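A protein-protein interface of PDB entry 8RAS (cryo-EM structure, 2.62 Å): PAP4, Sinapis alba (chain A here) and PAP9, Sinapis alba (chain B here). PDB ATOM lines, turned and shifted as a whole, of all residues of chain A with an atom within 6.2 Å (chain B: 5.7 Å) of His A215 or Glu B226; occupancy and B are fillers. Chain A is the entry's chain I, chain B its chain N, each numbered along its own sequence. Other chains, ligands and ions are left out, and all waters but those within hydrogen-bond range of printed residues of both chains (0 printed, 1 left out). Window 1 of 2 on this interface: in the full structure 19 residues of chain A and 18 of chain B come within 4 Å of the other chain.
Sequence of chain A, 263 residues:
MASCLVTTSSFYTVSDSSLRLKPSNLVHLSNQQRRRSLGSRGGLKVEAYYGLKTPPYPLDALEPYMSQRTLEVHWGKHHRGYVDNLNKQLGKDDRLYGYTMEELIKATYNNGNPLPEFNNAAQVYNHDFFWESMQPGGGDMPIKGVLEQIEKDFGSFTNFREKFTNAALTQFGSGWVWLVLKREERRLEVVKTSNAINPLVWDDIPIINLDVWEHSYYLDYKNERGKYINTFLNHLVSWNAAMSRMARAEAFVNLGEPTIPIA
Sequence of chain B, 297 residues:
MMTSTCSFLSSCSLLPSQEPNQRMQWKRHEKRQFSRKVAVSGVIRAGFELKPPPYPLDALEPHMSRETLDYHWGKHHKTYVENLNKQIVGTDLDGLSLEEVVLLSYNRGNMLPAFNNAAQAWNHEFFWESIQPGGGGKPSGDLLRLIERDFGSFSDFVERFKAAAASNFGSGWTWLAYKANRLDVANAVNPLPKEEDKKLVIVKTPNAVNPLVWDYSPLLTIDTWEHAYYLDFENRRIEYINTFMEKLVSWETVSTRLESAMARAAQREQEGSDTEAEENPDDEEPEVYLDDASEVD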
ATOM      1  N   THR A  70      -2.267 -11.428   6.480  1.00  0.00           N
ATOM      2  CA  THR A  70      -0.948 -11.645   5.896  1.00  0.00           C
ATOM      3  C   THR A  70      -0.732 -13.116   5.558  1.00  0.00           C
ATOM      4  O   THR A  70      -0.167 -13.441   4.509  1.00  0.00           O
ATOM      5  CB  THR A  70       0.145 -11.151   6.844  1.00  0.00           C
ATOM      6  OG1 THR A  70       0.384 -12.137   7.857  1.00  0.00           O
ATOM      7  CG2 THR A  70      -0.265  -9.841   7.496  1.00  0.00           C
ATOM      8  N   VAL A  73      -2.551 -14.137   2.335  1.00  0.00           N
ATOM      9  CA  VAL A  73      -2.069 -13.542   1.094  1.00  0.00           C
ATOM     10  C   VAL A  73      -0.654 -14.036   0.816  1.00  0.00           C
ATOM     11  O   VAL A  73      -0.259 -14.194  -0.344  1.00  0.00           O
ATOM     12  CB  VAL A  73      -2.138 -12.002   1.144  1.00  0.00           C
ATOM     13  CG1 VAL A  73      -1.178 -11.436   2.180  1.00  0.00           C
ATOM     14  CG2 VAL A  73      -1.864 -11.407  -0.231  1.00  0.00           C
ATOM     15  N   HIS A  74       0.116 -14.296   1.877  1.00  0.00           N
ATOM     16  CA  HIS A  74       1.471 -14.807   1.700  1.00  0.00           C
ATOM     17  C   HIS A  74       1.468 -16.277   1.303  1.00  0.00           C
ATOM     18  O   HIS A  74       2.401 -16.741   0.638  1.00  0.00           O
ATOM     19  CB  HIS A  74       2.278 -14.605   2.984  1.00  0.00           C
ATOM     20  CG  HIS A  74       3.758 -14.572   2.772  1.00  0.00           C
ATOM     21  ND1 HIS A  74       4.639 -14.165   3.751  1.00  0.00           N
ATOM     22  CD2 HIS A  74       4.514 -14.896   1.697  1.00  0.00           C
ATOM     23  CE1 HIS A  74       5.874 -14.242   3.288  1.00  0.00           C
ATOM     24  NE2 HIS A  74       5.826 -14.682   2.044  1.00  0.00           N
ATOM     25  N   HIS A  78       0.464 -15.813  -2.872  1.00  0.00           N
ATOM     26  CA  HIS A  78       1.898 -15.603  -3.049  1.00  0.00           C
ATOM     27  C   HIS A  78       2.636 -16.932  -3.153  1.00  0.00           C
ATOM     28  O   HIS A  78       3.254 -17.238  -4.179  1.00  0.00           O
ATOM     29  CB  HIS A  78       2.453 -14.768  -1.894  1.00  0.00           C
ATOM     30  CG  HIS A  78       2.493 -13.298  -2.172  1.00  0.00           C
ATOM     31  ND1 HIS A  78       3.079 -12.769  -3.301  1.00  0.00           N
ATOM     32  CD2 HIS A  78       2.024 -12.244  -1.463  1.00  0.00           C
ATOM     33  CE1 HIS A  78       2.969 -11.453  -3.277  1.00  0.00           C
ATOM     34  NE2 HIS A  78       2.332 -11.109  -2.172  1.00  0.00           N
ATOM     35  N   TYR A  82       3.768 -19.141  -6.735  1.00  0.00           N
ATOM     36  CA  TYR A  82       5.087 -19.688  -7.036  1.00  0.00           C
ATOM     37  C   TYR A  82       5.012 -21.186  -7.307  1.00  0.00           C
ATOM     38  O   TYR A  82       5.693 -21.699  -8.202  1.00  0.00           O
ATOM     39  CB  TYR A  82       6.048 -19.402  -5.882  1.00  0.00           C
ATOM     40  CG  TYR A  82       6.522 -17.971  -5.791  1.00  0.00           C
ATOM     41  CD1 TYR A  82       7.131 -17.349  -6.873  1.00  0.00           C
ATOM     42  CD2 TYR A  82       6.377 -17.246  -4.616  1.00  0.00           C
ATOM     43  CE1 TYR A  82       7.571 -16.042  -6.789  1.00  0.00           C
ATOM     44  CE2 TYR A  82       6.813 -15.941  -4.524  1.00  0.00           C
ATOM     45  CZ  TYR A  82       7.409 -15.344  -5.612  1.00  0.00           C
ATOM     46  OH  TYR A  82       7.847 -14.041  -5.524  1.00  0.00           O
ATOM     47  N   GLN A 123      11.759 -19.877  -4.881  1.00  0.00           N
ATOM     48  CA  GLN A 123      10.841 -19.149  -4.012  1.00  0.00           C
ATOM     49  C   GLN A 123       9.960 -20.086  -3.195  1.00  0.00           C
ATOM     50  O   GLN A 123       9.651 -19.790  -2.037  1.00  0.00           O
ATOM     51  CB  GLN A 123       9.978 -18.192  -4.832  1.00  0.00           C
ATOM     52  CG  GLN A 123      10.589 -16.813  -5.007  1.00  0.00           C
ATOM     53  CD  GLN A 123      10.767 -16.079  -3.692  1.00  0.00           C
ATOM     54  OE1 GLN A 123      11.814 -16.171  -3.053  1.00  0.00           O
ATOM     55  NE2 GLN A 123       9.743 -15.342  -3.282  1.00  0.00           N
ATOM     56  N   HIS A 127       9.730 -20.383   1.108  1.00  0.00           N
ATOM     57  CA  HIS A 127       8.498 -20.158   1.860  1.00  0.00           C
ATOM     58  C   HIS A 127       8.214 -21.301   2.830  1.00  0.00           C
ATOM     59  O   HIS A 127       7.895 -21.062   4.001  1.00  0.00           O
ATOM     60  CB  HIS A 127       7.332 -19.941   0.899  1.00  0.00           C
ATOM     61  CG  HIS A 127       7.278 -18.557   0.330  1.00  0.00           C
ATOM     62  ND1 HIS A 127       8.184 -18.099  -0.603  1.00  0.00           N
ATOM     63  CD2 HIS A 127       6.439 -17.524   0.577  1.00  0.00           C
ATOM     64  CE1 HIS A 127       7.899 -16.847  -0.912  1.00  0.00           C
ATOM     65  NE2 HIS A 127       6.844 -16.474  -0.211  1.00  0.00           N
ATOM     66  N   SER A 174      13.530  -6.298  -1.872  1.00  0.00           N
ATOM     67  CA  SER A 174      13.017  -7.616  -1.525  1.00  0.00           C
ATOM     68  C   SER A 174      14.151  -8.630  -1.479  1.00  0.00           C
ATOM     69  O   SER A 174      14.976  -8.699  -2.396  1.00  0.00           O
ATOM     70  CB  SER A 174      11.958  -8.050  -2.535  1.00  0.00           C
ATOM     71  OG  SER A 174      12.420  -7.859  -3.861  1.00  0.00           O
ATOM     72  N   ASP A 211      11.860 -13.526   6.113  1.00  0.00           N
ATOM     73  CA  ASP A 211      11.453 -12.915   4.855  1.00  0.00           C
ATOM     74  C   ASP A 211      11.367 -11.406   5.040  1.00  0.00           C
ATOM     75  O   ASP A 211      10.579 -10.921   5.858  1.00  0.00           O
ATOM     76  CB  ASP A 211      10.110 -13.473   4.386  1.00  0.00           C
ATOM     77  CG  ASP A 211       9.851 -13.210   2.915  1.00  0.00           C
ATOM     78  OD1 ASP A 211      10.725 -12.612   2.257  1.00  0.00           O
ATOM     79  OD2 ASP A 211       8.775 -13.602   2.418  1.00  0.00           O
ATOM     80  N   VAL A 212      12.176 -10.669   4.281  1.00  0.00           N
ATOM     81  CA  VAL A 212      12.134  -9.213   4.288  1.00  0.00           C
ATOM     82  C   VAL A 212      11.516  -8.664   3.010  1.00  0.00           C
ATOM     83  O   VAL A 212      11.651  -7.469   2.725  1.00  0.00           O
ATOM     84  CB  VAL A 212      13.525  -8.607   4.534  1.00  0.00           C
ATOM     85  CG1 VAL A 212      13.980  -8.892   5.957  1.00  0.00           C
ATOM     86  CG2 VAL A 212      14.527  -9.140   3.533  1.00  0.00           C
ATOM     87  N   TRP A 213      10.851  -9.509   2.223  1.00  0.00           N
ATOM     88  CA  TRP A 213      10.029  -9.012   1.130  1.00  0.00           C
ATOM     89  C   TRP A 213       8.921  -8.134   1.691  1.00  0.00           C
ATOM     90  O   TRP A 213       8.348  -8.428   2.743  1.00  0.00           O
ATOM     91  CB  TRP A 213       9.428 -10.172   0.333  1.00  0.00           C
ATOM     92  CG  TRP A 213      10.353 -10.780  -0.679  1.00  0.00           C
ATOM     93  CD1 TRP A 213      11.578 -11.327  -0.443  1.00  0.00           C
ATOM     94  CD2 TRP A 213      10.119 -10.918  -2.087  1.00  0.00           C
ATOM     95  NE1 TRP A 213      12.126 -11.789  -1.614  1.00  0.00           N
ATOM     96  CE2 TRP A 213      11.249 -11.550  -2.638  1.00  0.00           C
ATOM     97  CE3 TRP A 213       9.066 -10.561  -2.934  1.00  0.00           C
ATOM     98  CZ2 TRP A 213      11.356 -11.836  -3.998  1.00  0.00           C
ATOM     99  CZ3 TRP A 213       9.172 -10.848  -4.283  1.00  0.00           C
ATOM    100  CH2 TRP A 213      10.309 -11.478  -4.801  1.00  0.00           C
ATOM    101  N   GLU A 214       8.620  -7.045   0.981  1.00  0.00           N
ATOM    102  CA  GLU A 214       7.641  -6.088   1.484  1.00  0.00           C
ATOM    103  C   GLU A 214       6.273  -6.732   1.663  1.00  0.00           C
ATOM    104  O   GLU A 214       5.587  -6.481   2.659  1.00  0.00           O
ATOM    105  CB  GLU A 214       7.553  -4.884   0.547  1.00  0.00           C
ATOM    106  CG  GLU A 214       8.734  -3.936   0.661  1.00  0.00           C
ATOM    107  CD  GLU A 214       8.579  -2.707  -0.206  1.00  0.00           C
ATOM    108  OE1 GLU A 214       7.970  -2.817  -1.291  1.00  0.00           O
ATOM    109  OE2 GLU A 214       9.063  -1.628   0.199  1.00  0.00           O
ATOM    110  N   HIS A 215       5.869  -7.586   0.719  1.00  0.00           N
ATOM    111  CA  HIS A 215       4.559  -8.223   0.797  1.00  0.00           C
ATOM    112  C   HIS A 215       4.404  -9.095   2.036  1.00  0.00           C
ATOM    113  O   HIS A 215       3.273  -9.401   2.427  1.00  0.00           O
ATOM    114  CB  HIS A 215       4.307  -9.057  -0.459  1.00  0.00           C
ATOM    115  CG  HIS A 215       5.108 -10.320  -0.521  1.00  0.00           C
ATOM    116  ND1 HIS A 215       4.688 -11.499   0.055  1.00  0.00           N
ATOM    117  CD2 HIS A 215       6.303 -10.588  -1.099  1.00  0.00           C
ATOM    118  CE1 HIS A 215       5.591 -12.438  -0.163  1.00  0.00           C
ATOM    119  NE2 HIS A 215       6.581 -11.913  -0.860  1.00  0.00           N
ATOM    120  N   SER A 216       5.511  -9.502   2.662  1.00  0.00           N
ATOM    121  CA  SER A 216       5.418 -10.357   3.840  1.00  0.00           C
ATOM    122  C   SER A 216       4.968  -9.584   5.073  1.00  0.00           C
ATOM    123  O   SER A 216       4.340 -10.164   5.967  1.00  0.00           O
ATOM    124  CB  SER A 216       6.762 -11.034   4.103  1.00  0.00           C
ATOM    125  OG  SER A 216       7.811 -10.084   4.142  1.00  0.00           O
ATOM    126  N   TYR A 217       5.277  -8.284   5.148  1.00  0.00           N
ATOM    127  CA  TYR A 217       4.998  -7.530   6.364  1.00  0.00           C
ATOM    128  C   TYR A 217       4.453  -6.128   6.096  1.00  0.00           C
ATOM    129  O   TYR A 217       4.537  -5.267   6.981  1.00  0.00           O
ATOM    130  CB  TYR A 217       6.260  -7.424   7.229  1.00  0.00           C
ATOM    131  CG  TYR A 217       7.401  -6.681   6.565  1.00  0.00           C
ATOM    132  CD1 TYR A 217       8.261  -7.328   5.690  1.00  0.00           C
ATOM    133  CD2 TYR A 217       7.617  -5.332   6.817  1.00  0.00           C
ATOM    134  CE1 TYR A 217       9.303  -6.652   5.082  1.00  0.00           C
ATOM    135  CE2 TYR A 217       8.654  -4.650   6.213  1.00  0.00           C
ATOM    136  CZ  TYR A 217       9.494  -5.315   5.346  1.00  0.00           C
ATOM    137  OH  TYR A 217      10.528  -4.637   4.743  1.00  0.00           O
ATOM    138  N   TYR A 218       3.885  -5.871   4.918  1.00  0.00           N
ATOM    139  CA  TYR A 218       3.424  -4.523   4.606  1.00  0.00           C
ATOM    140  C   TYR A 218       2.019  -4.233   5.119  1.00  0.00           C
ATOM    141  O   TYR A 218       1.494  -3.149   4.852  1.00  0.00           O
ATOM    142  CB  TYR A 218       3.471  -4.267   3.097  1.00  0.00           C
ATOM    143  CG  TYR A 218       3.641  -2.804   2.754  1.00  0.00           C
ATOM    144  CD1 TYR A 218       4.785  -2.115   3.130  1.00  0.00           C
ATOM    145  CD2 TYR A 218       2.651  -2.108   2.074  1.00  0.00           C
ATOM    146  CE1 TYR A 218       4.945  -0.777   2.831  1.00  0.00           C
ATOM    147  CE2 TYR A 218       2.801  -0.768   1.770  1.00  0.00           C
ATOM    148  CZ  TYR A 218       3.950  -0.108   2.151  1.00  0.00           C
ATOM    149  OH  TYR A 218       4.108   1.224   1.849  1.00  0.00           O
ATOM    150  N   LEU A 219       1.394  -5.165   5.834  1.00  0.00           N
ATOM    151  CA  LEU A 219       0.073  -4.932   6.402  1.00  0.00           C
ATOM    152  C   LEU A 219       0.116  -4.560   7.877  1.00  0.00           C
ATOM    153  O   LEU A 219      -0.582  -3.631   8.296  1.00  0.00           O
ATOM    154  CB  LEU A 219      -0.812  -6.167   6.216  1.00  0.00           C
ATOM    155  CG  LEU A 219      -1.834  -6.081   5.083  1.00  0.00           C
ATOM    156  CD1 LEU A 219      -1.141  -5.860   3.750  1.00  0.00           C
ATOM    157  CD2 LEU A 219      -2.693  -7.331   5.041  1.00  0.00           C
ATOM    158  N   SER B 171      11.418  -6.209  -5.876  1.00  0.00           N
ATOM    159  CA  SER B 171      11.321  -4.757  -5.875  1.00  0.00           C
ATOM    160  C   SER B 171      12.077  -4.172  -7.062  1.00  0.00           C
ATOM    161  O   SER B 171      13.191  -4.598  -7.381  1.00  0.00           O
ATOM    162  CB  SER B 171      11.872  -4.190  -4.569  1.00  0.00           C
ATOM    163  OG  SER B 171      11.161  -4.695  -3.453  1.00  0.00           O
ATOM    164  N   THR B 224       6.963  -0.788  -9.455  1.00  0.00           N
ATOM    165  CA  THR B 224       6.640  -2.188  -9.229  1.00  0.00           C
ATOM    166  C   THR B 224       7.006  -2.650  -7.826  1.00  0.00           C
ATOM    167  O   THR B 224       6.772  -3.816  -7.492  1.00  0.00           O
ATOM    168  CB  THR B 224       7.339  -3.076 -10.263  1.00  0.00           C
ATOM    169  OG1 THR B 224       8.709  -3.265  -9.889  1.00  0.00           O
ATOM    170  CG2 THR B 224       7.277  -2.437 -11.642  1.00  0.00           C
ATOM    171  N   TRP B 225       7.585  -1.771  -7.009  1.00  0.00           N
ATOM    172  CA  TRP B 225       7.774  -2.073  -5.598  1.00  0.00           C
ATOM    173  C   TRP B 225       6.433  -2.385  -4.953  1.00  0.00           C
ATOM    174  O   TRP B 225       5.437  -1.694  -5.186  1.00  0.00           O
ATOM    175  CB  TRP B 225       8.427  -0.893  -4.881  1.00  0.00           C
ATOM    176  CG  TRP B 225       9.911  -0.817  -5.020  1.00  0.00           C
ATOM    177  CD1 TRP B 225      10.621  -0.657  -6.170  1.00  0.00           C
ATOM    178  CD2 TRP B 225      10.870  -0.884  -3.959  1.00  0.00           C
ATOM    179  NE1 TRP B 225      11.966  -0.627  -5.896  1.00  0.00           N
ATOM    180  CE2 TRP B 225      12.146  -0.762  -4.544  1.00  0.00           C
ATOM    181  CE3 TRP B 225      10.776  -1.037  -2.574  1.00  0.00           C
ATOM    182  CZ2 TRP B 225      13.317  -0.791  -3.791  1.00  0.00           C
ATOM    183  CZ3 TRP B 225      11.938  -1.065  -1.829  1.00  0.00           C
ATOM    184  CH2 TRP B 225      13.191  -0.943  -2.438  1.00  0.00           C
ATOM    185  N   GLU B 226       6.411  -3.434  -4.129  1.00  0.00           N
ATOM    186  CA  GLU B 226       5.156  -3.866  -3.526  1.00  0.00           C
ATOM    187  C   GLU B 226       4.586  -2.810  -2.587  1.00  0.00           C
ATOM    188  O   GLU B 226       3.366  -2.744  -2.404  1.00  0.00           O
ATOM    189  CB  GLU B 226       5.362  -5.189  -2.795  1.00  0.00           C
ATOM    190  CG  GLU B 226       5.751  -6.329  -3.721  1.00  0.00           C
ATOM    191  CD  GLU B 226       6.111  -7.594  -2.975  1.00  0.00           C
ATOM    192  OE1 GLU B 226       6.788  -7.497  -1.930  1.00  0.00           O
ATOM    193  OE2 GLU B 226       5.716  -8.686  -3.434  1.00  0.00           O
ATOM    194  N   HIS B 227       5.441  -1.969  -2.002  1.00  0.00           N
ATOM    195  CA  HIS B 227       4.956  -0.911  -1.123  1.00  0.00           C
ATOM    196  C   HIS B 227       4.124   0.127  -1.864  1.00  0.00           C
ATOM    197  O   HIS B 227       3.376   0.874  -1.226  1.00  0.00           O
ATOM    198  CB  HIS B 227       6.133  -0.232  -0.416  1.00  0.00           C
ATOM    199  CG  HIS B 227       6.773   0.864  -1.209  1.00  0.00           C
ATOM    200  ND1 HIS B 227       7.805   0.636  -2.093  1.00  0.00           N
ATOM    201  CD2 HIS B 227       6.538   2.197  -1.242  1.00  0.00           C
ATOM    202  CE1 HIS B 227       8.173   1.781  -2.642  1.00  0.00           C
ATOM    203  NE2 HIS B 227       7.420   2.742  -2.142  1.00  0.00           N
ATOM    204  N   ALA B 228       4.234   0.190  -3.193  1.00  0.00           N
ATOM    205  CA  ALA B 228       3.481   1.182  -3.951  1.00  0.00           C
ATOM    206  C   ALA B 228       2.008   0.810  -4.078  1.00  0.00           C
ATOM    207  O   ALA B 228       1.160   1.699  -4.220  1.00  0.00           O
ATOM    208  CB  ALA B 228       4.100   1.364  -5.337  1.00  0.00           C
ATOM    209  N   TYR B 229       1.679  -0.483  -4.032  1.00  0.00           N
ATOM    210  CA  TYR B 229       0.315  -0.915  -4.300  1.00  0.00           C
ATOM    211  C   TYR B 229      -0.218  -1.977  -3.348  1.00  0.00           C
ATOM    212  O   TYR B 229      -1.372  -2.385  -3.504  1.00  0.00           O
ATOM    213  CB  TYR B 229       0.199  -1.442  -5.741  1.00  0.00           C
ATOM    214  CG  TYR B 229       1.231  -2.489  -6.094  1.00  0.00           C
ATOM    215  CD1 TYR B 229       0.991  -3.836  -5.859  1.00  0.00           C
ATOM    216  CD2 TYR B 229       2.445  -2.130  -6.666  1.00  0.00           C
ATOM    217  CE1 TYR B 229       1.931  -4.795  -6.180  1.00  0.00           C
ATOM    218  CE2 TYR B 229       3.390  -3.083  -6.991  1.00  0.00           C
ATOM    219  CZ  TYR B 229       3.128  -4.413  -6.745  1.00  0.00           C
ATOM    220  OH  TYR B 229       4.067  -5.365  -7.067  1.00  0.00           O
ATOM    221  N   TYR B 230       0.571  -2.443  -2.375  1.00  0.00           N
ATOM    222  CA  TYR B 230       0.095  -3.516  -1.505  1.00  0.00           C
ATOM    223  C   TYR B 230      -1.077  -3.072  -0.642  1.00  0.00           C
ATOM    224  O   TYR B 230      -1.914  -3.901  -0.266  1.00  0.00           O
ATOM    225  CB  TYR B 230       1.230  -4.033  -0.622  1.00  0.00           C
ATOM    226  CG  TYR B 230       1.145  -5.515  -0.350  1.00  0.00           C
ATOM    227  CD1 TYR B 230       1.228  -6.434  -1.387  1.00  0.00           C
ATOM    228  CD2 TYR B 230       0.974  -5.998   0.939  1.00  0.00           C
ATOM    229  CE1 TYR B 230       1.143  -7.789  -1.150  1.00  0.00           C
ATOM    230  CE2 TYR B 230       0.891  -7.354   1.188  1.00  0.00           C
ATOM    231  CZ  TYR B 230       0.977  -8.245   0.140  1.00  0.00           C
ATOM    232  OH  TYR B 230       0.896  -9.596   0.380  1.00  0.00           O
ATOM    233  N   LEU B 231      -1.156  -1.782  -0.314  1.00  0.00           N
ATOM    234  CA  LEU B 231      -2.245  -1.310   0.531  1.00  0.00           C
ATOM    235  C   LEU B 231      -3.581  -1.324  -0.202  1.00  0.00           C
ATOM    236  O   LEU B 231      -4.628  -1.512   0.428  1.00  0.00           O
ATOM    237  CB  LEU B 231      -1.935   0.092   1.048  1.00  0.00           C
ATOM    238  CG  LEU B 231      -0.859   0.165   2.131  1.00  0.00           C
ATOM    239  CD1 LEU B 231      -0.495   1.609   2.436  1.00  0.00           C
ATOM    240  CD2 LEU B 231      -1.327  -0.558   3.381  1.00  0.00           C
ATOM    241  N   GLU B 234      -3.018  -5.141  -3.040  1.00  0.00           N
ATOM    242  CA  GLU B 234      -2.383  -6.297  -2.389  1.00  0.00           C
ATOM    243  C   GLU B 234      -1.387  -6.901  -3.381  1.00  0.00           C
ATOM    244  O   GLU B 234      -0.557  -6.164  -3.928  1.00  0.00           O
ATOM    245  CB  GLU B 234      -3.461  -7.243  -1.879  1.00  0.00           C
ATOM    246  CG  GLU B 234      -3.883  -6.987  -0.441  1.00  0.00           C
ATOM    247  CD  GLU B 234      -5.002  -7.904   0.009  1.00  0.00           C
ATOM    248  OE1 GLU B 234      -5.743  -8.412  -0.860  1.00  0.00           O
ATOM    249  OE2 GLU B 234      -5.143  -8.118   1.231  1.00  0.00           O
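Among the printed residues, merely in contact across the chains: Val A73 with Tyr B230 (3.3 Å), His A78 with Glu B226 (3.9 Å), Trp A213 with Glu B226 (3.9 Å), Glu A214 with Trp B225 (3.3 Å), Tyr A218 with Tyr B230 (3.6 Å), Tyr A218 with Leu B231 (3.8 Å) and Leu A219 with Tyr B230 (3.5 Å).
Val A212 touches none of the printed residues of chain B.
Of chain B, only Glu B226 (2.8 Å) and Tyr B230 (3.1 Å) come within 4 Å of His A215.
Of the printed residues of chain B, Tyr A218 touches His B227 (3.2 Å), Tyr B230 (3.6 Å) and Leu B231 (3.8 Å).
Of the printed residues of chain A, Glu B226 touches His A78 (3.9 Å), Trp A213 (3.9 Å), Glu A214 (3.3 Å) and His A215 (2.8 Å).
Of the printed residues of chain A, His B227 touches Glu A214 and Tyr A218.
Ala B228 touches none of the printed residues of chain A.
Printed residues of chain A within 4 Å of Tyr B230: Val A73, His A78, His A215, Tyr A218 and Leu A219.
The nearest residue of chain A that does not touch Glu B226 is Tyr A218 (4.6 Å).
The side-chain carboxylate (OE1) of Glu A214 sits at hydrogen-bond distance from the backbone NH (N) of His B227 (2.8 Å).
OH of Tyr A218 is in hydrogen-bond range of O of His B227 (3.2 Å).
OH of Tyr B230 sits at hydrogen-bond distance from O of His A215 (3.1 Å).
N of Ser B171 sits at hydrogen-bond distance from OG of Ser A174, 2.8 Å away.
The side-chain carboxylate (OE1) of Glu B226 lies within hydrogen-bond range of the backbone NH (N) of His A215, 2.8 Å away.
N of Glu B226 sits at hydrogen-bond distance from OE1 of Glu A214 (3.3 Å).
A ring nitrogen (NE2) of His A78 is in hydrogen-bond range of the side-chain hydroxyl of Tyr B230 (3.3 Å).
Of the 17 printed residues of chain A, 8 touch a printed residue of chain B.
Hydrophobic or aromatic side chains of chain A that line the printed part of chain B: Val A73, His A78, Trp A213, His A215, Tyr A218 and Leu A219.
Printed residues of chain B that touch a printed residue of chain A: Ser B171, Trp B225, Glu B226, His B227, Tyr B230 and Leu B231.
Hydrophobic or aromatic side chains of chain B that line the printed part of chain A: Trp B225, His B227, Tyr B230 and Leu B231.
Among the printed residues, no Asp or Glu carboxylate lies within 4 Å of a Lys or Arg side-chain nitrogen of the other chain.
A ring nitrogen (NE2) of His A78 sits close to a ring nitrogen (ND1) of His A215 (3.3 Å).
OD1 of Asp A211 is in hydrogen-bond range of N of Trp A213, at 3.1 Å.
N of His A78 lies within hydrogen-bond range of O of Val A73 (3.1 Å).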
